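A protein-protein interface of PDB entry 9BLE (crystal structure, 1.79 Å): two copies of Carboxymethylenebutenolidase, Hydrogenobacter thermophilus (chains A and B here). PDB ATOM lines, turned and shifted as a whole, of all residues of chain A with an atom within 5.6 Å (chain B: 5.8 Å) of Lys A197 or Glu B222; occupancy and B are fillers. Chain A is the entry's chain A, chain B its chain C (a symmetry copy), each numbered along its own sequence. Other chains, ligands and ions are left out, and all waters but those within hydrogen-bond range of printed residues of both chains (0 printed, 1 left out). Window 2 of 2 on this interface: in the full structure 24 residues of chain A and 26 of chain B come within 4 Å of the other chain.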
ATOM      1  N   ALA A 166      23.674  26.088 -36.973  1.00  0.00           N
ATOM      2  CA  ALA A 166      22.546  25.489 -36.262  1.00  0.00           C
ATOM      3  C   ALA A 166      22.759  25.549 -34.755  1.00  0.00           C
ATOM      4  O   ALA A 166      23.889  25.570 -34.282  1.00  0.00           O
ATOM      5  CB  ALA A 166      22.351  24.055 -36.696  1.00  0.00           C
ATOM      6  N   PRO A 167      21.679  25.514 -33.940  1.00  0.00           N
ATOM      7  CA  PRO A 167      21.806  25.222 -32.520  1.00  0.00           C
ATOM      8  C   PRO A 167      22.267  23.783 -32.320  1.00  0.00           C
ATOM      9  O   PRO A 167      21.912  22.906 -33.111  1.00  0.00           O
ATOM     10  CB  PRO A 167      20.402  25.462 -31.963  1.00  0.00           C
ATOM     11  CG  PRO A 167      19.484  25.230 -33.133  1.00  0.00           C
ATOM     12  CD  PRO A 167      20.279  25.696 -34.367  1.00  0.00           C
ATOM     13  N   VAL A 168      23.028  23.565 -31.246  1.00  0.00           N
ATOM     14  CA  VAL A 168      23.668  22.292 -30.955  1.00  0.00           C
ATOM     15  C   VAL A 168      23.312  21.871 -29.531  1.00  0.00           C
ATOM     16  O   VAL A 168      23.374  22.657 -28.597  1.00  0.00           O
ATOM     17  CB  VAL A 168      25.195  22.356 -31.114  1.00  0.00           C
ATOM     18  CG1 VAL A 168      25.870  21.015 -30.884  1.00  0.00           C
ATOM     19  CG2 VAL A 168      25.594  22.925 -32.471  1.00  0.00           C
ATOM     20  N   LEU A 169      22.915  20.607 -29.391  1.00  0.00           N
ATOM     21  CA  LEU A 169      22.824  19.934 -28.099  1.00  0.00           C
ATOM     22  C   LEU A 169      23.894  18.841 -28.072  1.00  0.00           C
ATOM     23  O   LEU A 169      23.745  17.816 -28.716  1.00  0.00           O
ATOM     24  CB  LEU A 169      21.419  19.364 -27.928  1.00  0.00           C
ATOM     25  CG  LEU A 169      21.205  18.387 -26.761  1.00  0.00           C
ATOM     26  CD1 LEU A 169      21.598  18.993 -25.485  1.00  0.00           C
ATOM     27  CD2 LEU A 169      19.779  17.983 -26.634  1.00  0.00           C
ATOM     28  N   GLY A 195      30.526  32.113 -31.290  1.00  0.00           N
ATOM     29  CA  GLY A 195      29.110  32.426 -31.163  1.00  0.00           C
ATOM     30  C   GLY A 195      28.205  31.240 -31.530  1.00  0.00           C
ATOM     31  O   GLY A 195      27.059  31.437 -31.931  1.00  0.00           O
ATOM     32  N   VAL A 196      28.698  30.008 -31.372  1.00  0.00           N
ATOM     33  CA  VAL A 196      27.879  28.841 -31.663  1.00  0.00           C
ATOM     34  C   VAL A 196      26.876  28.662 -30.526  1.00  0.00           C
ATOM     35  O   VAL A 196      27.245  28.683 -29.353  1.00  0.00           O
ATOM     36  CB  VAL A 196      28.713  27.568 -31.845  1.00  0.00           C
ATOM     37  CG1 VAL A 196      27.819  26.359 -32.142  1.00  0.00           C
ATOM     38  CG2 VAL A 196      29.779  27.750 -32.925  1.00  0.00           C
ATOM     39  N   LYS A 197      25.597  28.495 -30.889  1.00  0.00           N
ATOM     40  CA  LYS A 197      24.529  28.313 -29.919  1.00  0.00           C
ATOM     41  C   LYS A 197      24.499  26.848 -29.486  1.00  0.00           C
ATOM     42  O   LYS A 197      23.601  26.089 -29.862  1.00  0.00           O
ATOM     43  CB  LYS A 197      23.262  28.824 -30.601  1.00  0.00           C
ATOM     44  CG  LYS A 197      22.083  29.145 -29.750  1.00  0.00           C
ATOM     45  CD  LYS A 197      20.873  28.518 -30.433  1.00  0.00           C
ATOM     46  CE  LYS A 197      19.534  28.974 -30.003  1.00  0.00           C
ATOM     47  NZ  LYS A 197      18.527  28.261 -30.789  1.00  0.00           N
ATOM     48  N   ALA A 198      25.488  26.488 -28.668  1.00  0.00           N
ATOM     49  CA  ALA A 198      25.690  25.123 -28.232  1.00  0.00           C
ATOM     50  C   ALA A 198      25.419  24.999 -26.737  1.00  0.00           C
ATOM     51  O   ALA A 198      25.974  25.740 -25.919  1.00  0.00           O
ATOM     52  CB  ALA A 198      27.075  24.652 -28.573  1.00  0.00           C
ATOM     53  N   GLN A 199      24.571  24.026 -26.390  1.00  0.00           N
ATOM     54  CA  GLN A 199      24.424  23.599 -25.016  1.00  0.00           C
ATOM     55  C   GLN A 199      25.102  22.239 -24.839  1.00  0.00           C
ATOM     56  O   GLN A 199      24.908  21.339 -25.659  1.00  0.00           O
ATOM     57  CB  GLN A 199      22.957  23.650 -24.636  1.00  0.00           C
ATOM     58  CG  GLN A 199      22.070  22.684 -25.400  1.00  0.00           C
ATOM     59  CD  GLN A 199      20.602  22.856 -25.083  1.00  0.00           C
ATOM     60  OE1 GLN A 199      20.023  22.033 -24.375  1.00  0.00           O
ATOM     61  NE2 GLN A 199      19.987  23.896 -25.636  1.00  0.00           N
ATOM     62  N   HIS A 238      13.292  23.195 -32.272  1.00  0.00           N
ATOM     63  CA  HIS A 238      13.967  23.790 -33.413  1.00  0.00           C
ATOM     64  C   HIS A 238      13.455  23.314 -34.772  1.00  0.00           C
ATOM     65  O   HIS A 238      13.730  23.973 -35.779  1.00  0.00           O
ATOM     66  CB  HIS A 238      15.478  23.591 -33.283  1.00  0.00           C
ATOM     67  CG  HIS A 238      15.990  24.402 -32.160  1.00  0.00           C
ATOM     68  ND1 HIS A 238      16.473  23.867 -30.981  1.00  0.00           N
ATOM     69  CD2 HIS A 238      16.037  25.719 -32.046  1.00  0.00           C
ATOM     70  CE1 HIS A 238      16.830  24.851 -30.194  1.00  0.00           C
ATOM     71  NE2 HIS A 238      16.594  25.983 -30.827  1.00  0.00           N
ATOM     72  N   SER B 204      26.753  27.770 -23.927  1.00  0.00           N
ATOM     73  CA  SER B 204      27.777  28.582 -24.560  1.00  0.00           C
ATOM     74  C   SER B 204      27.304  30.014 -24.707  1.00  0.00           C
ATOM     75  O   SER B 204      26.121  30.256 -24.974  1.00  0.00           O
ATOM     76  CB  SER B 204      28.109  28.040 -25.935  1.00  0.00           C
ATOM     77  OG  SER B 204      28.573  26.708 -25.807  1.00  0.00           O
ATOM     78  N   ASN B 220      19.430  36.164 -20.988  1.00  0.00           N
ATOM     79  CA  ASN B 220      19.349  35.575 -22.306  1.00  0.00           C
ATOM     80  C   ASN B 220      18.024  34.841 -22.401  1.00  0.00           C
ATOM     81  O   ASN B 220      17.877  33.776 -21.821  1.00  0.00           O
ATOM     82  CB  ASN B 220      20.525  34.645 -22.601  1.00  0.00           C
ATOM     83  CG  ASN B 220      20.497  34.169 -24.036  1.00  0.00           C
ATOM     84  OD1 ASN B 220      19.862  33.162 -24.368  1.00  0.00           O
ATOM     85  ND2 ASN B 220      21.195  34.889 -24.903  1.00  0.00           N
ATOM     86  N   GLU B 221      17.087  35.400 -23.173  1.00  0.00           N
ATOM     87  CA  GLU B 221      15.726  34.888 -23.239  1.00  0.00           C
ATOM     88  C   GLU B 221      15.702  33.441 -23.715  1.00  0.00           C
ATOM     89  O   GLU B 221      15.047  32.587 -23.120  1.00  0.00           O
ATOM     90  CB  GLU B 221      14.812  35.710 -24.145  1.00  0.00           C
ATOM     91  CG  GLU B 221      13.364  35.226 -24.085  1.00  0.00           C
ATOM     92  CD  GLU B 221      12.398  36.120 -24.844  1.00  0.00           C
ATOM     93  OE1 GLU B 221      12.633  36.280 -26.056  1.00  0.00           O
ATOM     94  OE2 GLU B 221      11.441  36.674 -24.264  1.00  0.00           O
ATOM     95  N   GLU B 222      16.402  33.179 -24.817  1.00  0.00           N
ATOM     96  CA  GLU B 222      16.328  31.874 -25.450  1.00  0.00           C
ATOM     97  C   GLU B 222      16.801  30.769 -24.498  1.00  0.00           C
ATOM     98  O   GLU B 222      16.148  29.730 -24.367  1.00  0.00           O
ATOM     99  CB  GLU B 222      17.131  31.901 -26.746  1.00  0.00           C
ATOM    100  CG  GLU B 222      17.104  30.574 -27.489  1.00  0.00           C
ATOM    101  CD  GLU B 222      17.280  30.821 -28.984  1.00  0.00           C
ATOM    102  OE1 GLU B 222      18.198  31.611 -29.324  1.00  0.00           O
ATOM    103  OE2 GLU B 222      16.490  30.270 -29.791  1.00  0.00           O
ATOM    104  N   TYR B 223      17.938  30.985 -23.836  1.00  0.00           N
ATOM    105  CA  TYR B 223      18.445  29.966 -22.928  1.00  0.00           C
ATOM    106  C   TYR B 223      17.670  29.924 -21.615  1.00  0.00           C
ATOM    107  O   TYR B 223      17.610  28.858 -20.982  1.00  0.00           O
ATOM    108  CB  TYR B 223      19.950  30.141 -22.752  1.00  0.00           C
ATOM    109  CG  TYR B 223      20.760  29.584 -23.922  1.00  0.00           C
ATOM    110  CD1 TYR B 223      20.200  28.651 -24.798  1.00  0.00           C
ATOM    111  CD2 TYR B 223      22.095  29.920 -24.107  1.00  0.00           C
ATOM    112  CE1 TYR B 223      20.930  28.103 -25.839  1.00  0.00           C
ATOM    113  CE2 TYR B 223      22.840  29.371 -25.142  1.00  0.00           C
ATOM    114  CZ  TYR B 223      22.250  28.471 -26.013  1.00  0.00           C
ATOM    115  OH  TYR B 223      22.932  27.859 -27.021  1.00  0.00           O
ATOM    116  N   ALA B 224      17.140  31.071 -21.166  1.00  0.00           N
ATOM    117  CA  ALA B 224      16.323  31.083 -19.957  1.00  0.00           C
ATOM    118  C   ALA B 224      15.073  30.221 -20.174  1.00  0.00           C
ATOM    119  O   ALA B 224      14.660  29.487 -19.291  1.00  0.00           O
ATOM    120  CB  ALA B 224      15.919  32.501 -19.564  1.00  0.00           C
ATOM    121  N   VAL B 225      14.469  30.329 -21.364  1.00  0.00           N
ATOM    122  CA  VAL B 225      13.280  29.553 -21.669  1.00  0.00           C
ATOM    123  C   VAL B 225      13.642  28.073 -21.776  1.00  0.00           C
ATOM    124  O   VAL B 225      12.945  27.204 -21.253  1.00  0.00           O
ATOM    125  CB  VAL B 225      12.611  30.073 -22.946  1.00  0.00           C
ATOM    126  CG1 VAL B 225      11.520  29.122 -23.443  1.00  0.00           C
ATOM    127  CG2 VAL B 225      12.042  31.471 -22.710  1.00  0.00           C
ATOM    128  N   ASP B 226      14.774  27.791 -22.415  1.00  0.00           N
ATOM    129  CA  ASP B 226      15.263  26.427 -22.558  1.00  0.00           C
ATOM    130  C   ASP B 226      15.512  25.778 -21.192  1.00  0.00           C
ATOM    131  O   ASP B 226      15.057  24.653 -20.910  1.00  0.00           O
ATOM    132  CB  ASP B 226      16.519  26.408 -23.405  1.00  0.00           C
ATOM    133  CG  ASP B 226      17.091  25.019 -23.681  1.00  0.00           C
ATOM    134  OD1 ASP B 226      17.554  24.381 -22.713  1.00  0.00           O
ATOM    135  OD2 ASP B 226      17.055  24.579 -24.869  1.00  0.00           O
ATOM    136  N   VAL B 227      16.245  26.489 -20.327  1.00  0.00           N
ATOM    137  CA  VAL B 227      16.668  25.892 -19.070  1.00  0.00           C
ATOM    138  C   VAL B 227      15.467  25.716 -18.133  1.00  0.00           C
ATOM    139  O   VAL B 227      15.415  24.752 -17.372  1.00  0.00           O
ATOM    140  CB  VAL B 227      17.828  26.646 -18.401  1.00  0.00           C
ATOM    141  CG1 VAL B 227      17.416  27.976 -17.767  1.00  0.00           C
ATOM    142  CG2 VAL B 227      18.558  25.757 -17.399  1.00  0.00           C
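The side-chain amino group (NZ) of Lys A197 is in salt-bridge range of the side-chain carboxylate (OE2) of Glu B222 (3.0 Å).
The backbone carbonyl oxygen (O) of Lys A197 sits close to the side-chain hydroxyl (OH) of Tyr B223.
The backbone carbonyl oxygen (O) of Ala A198 sits at hydrogen-bond distance from the side-chain hydroxyl (OG) of Ser B204, at 2.8 Å.
The side-chain hydroxyl (OH) of Tyr B223 sits at hydrogen-bond distance from the backbone NH (N) of Ala A198 (3.3 Å).
OD2 of Asp B226 sits at hydrogen-bond distance from NE2 of Gln A199 (3.1 Å).
The backbone NH (N) of Val A168 is in hydrogen-bond range of the backbone carbonyl oxygen (O) of Lys A197 (2.9 Å).
O of Val A168 sits at hydrogen-bond distance from N of Gln A199.
NZ of Lys A197 lies within hydrogen-bond range of NE2 of His A238, at 3.0 Å.
The backbone NH (N) of Glu B222 lies close to the side-chain amide oxygen (OD1) of Asn B220 (3.5 Å).
OD1 of Asn B220 lies within hydrogen-bond range of N of Tyr B223.
O of Val A196 touches CB of Ser B204 (3.6 Å).
Of the printed residues of chain B, Val A196 touches Ser B204.
Of chain B, only Glu B222 (3.0 Å) and Tyr B223 (3.1 Å) come within 4 Å of Lys A197.
Of the printed residues of chain B, Gln A199 touches Asp B226.
Glu B221 touches none of the printed residues of chain A.
Glu B222 touches one residue of chain A.
Printed residues of chain A within 4 Å of Tyr B223: Lys A197 (3.1 Å) and Ala A198 (3.3 Å).
Printed residues of chain A within 4 Å of Asp B226: Gln A199 (3.1 Å).
Val B227 touches none of the printed residues of chain A.
The nearest residue of chain B that does not touch Lys A197 is Ser B204 (5.2 Å).
The nearest printed residue of chain B that does not touch Gln A199 is Tyr B223 (4.2 Å).
Hydrophobic or aromatic side chains of chain A within 4 Å of the printed part of chain B: Ala A198.
Of the 9 printed residues of chain B, 4 touch a printed residue of chain A.
No position is printed for both chains.
Of the 6 pairs that touch across the chains among the printed residues, none has its exchanged pair printed and touching as well.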
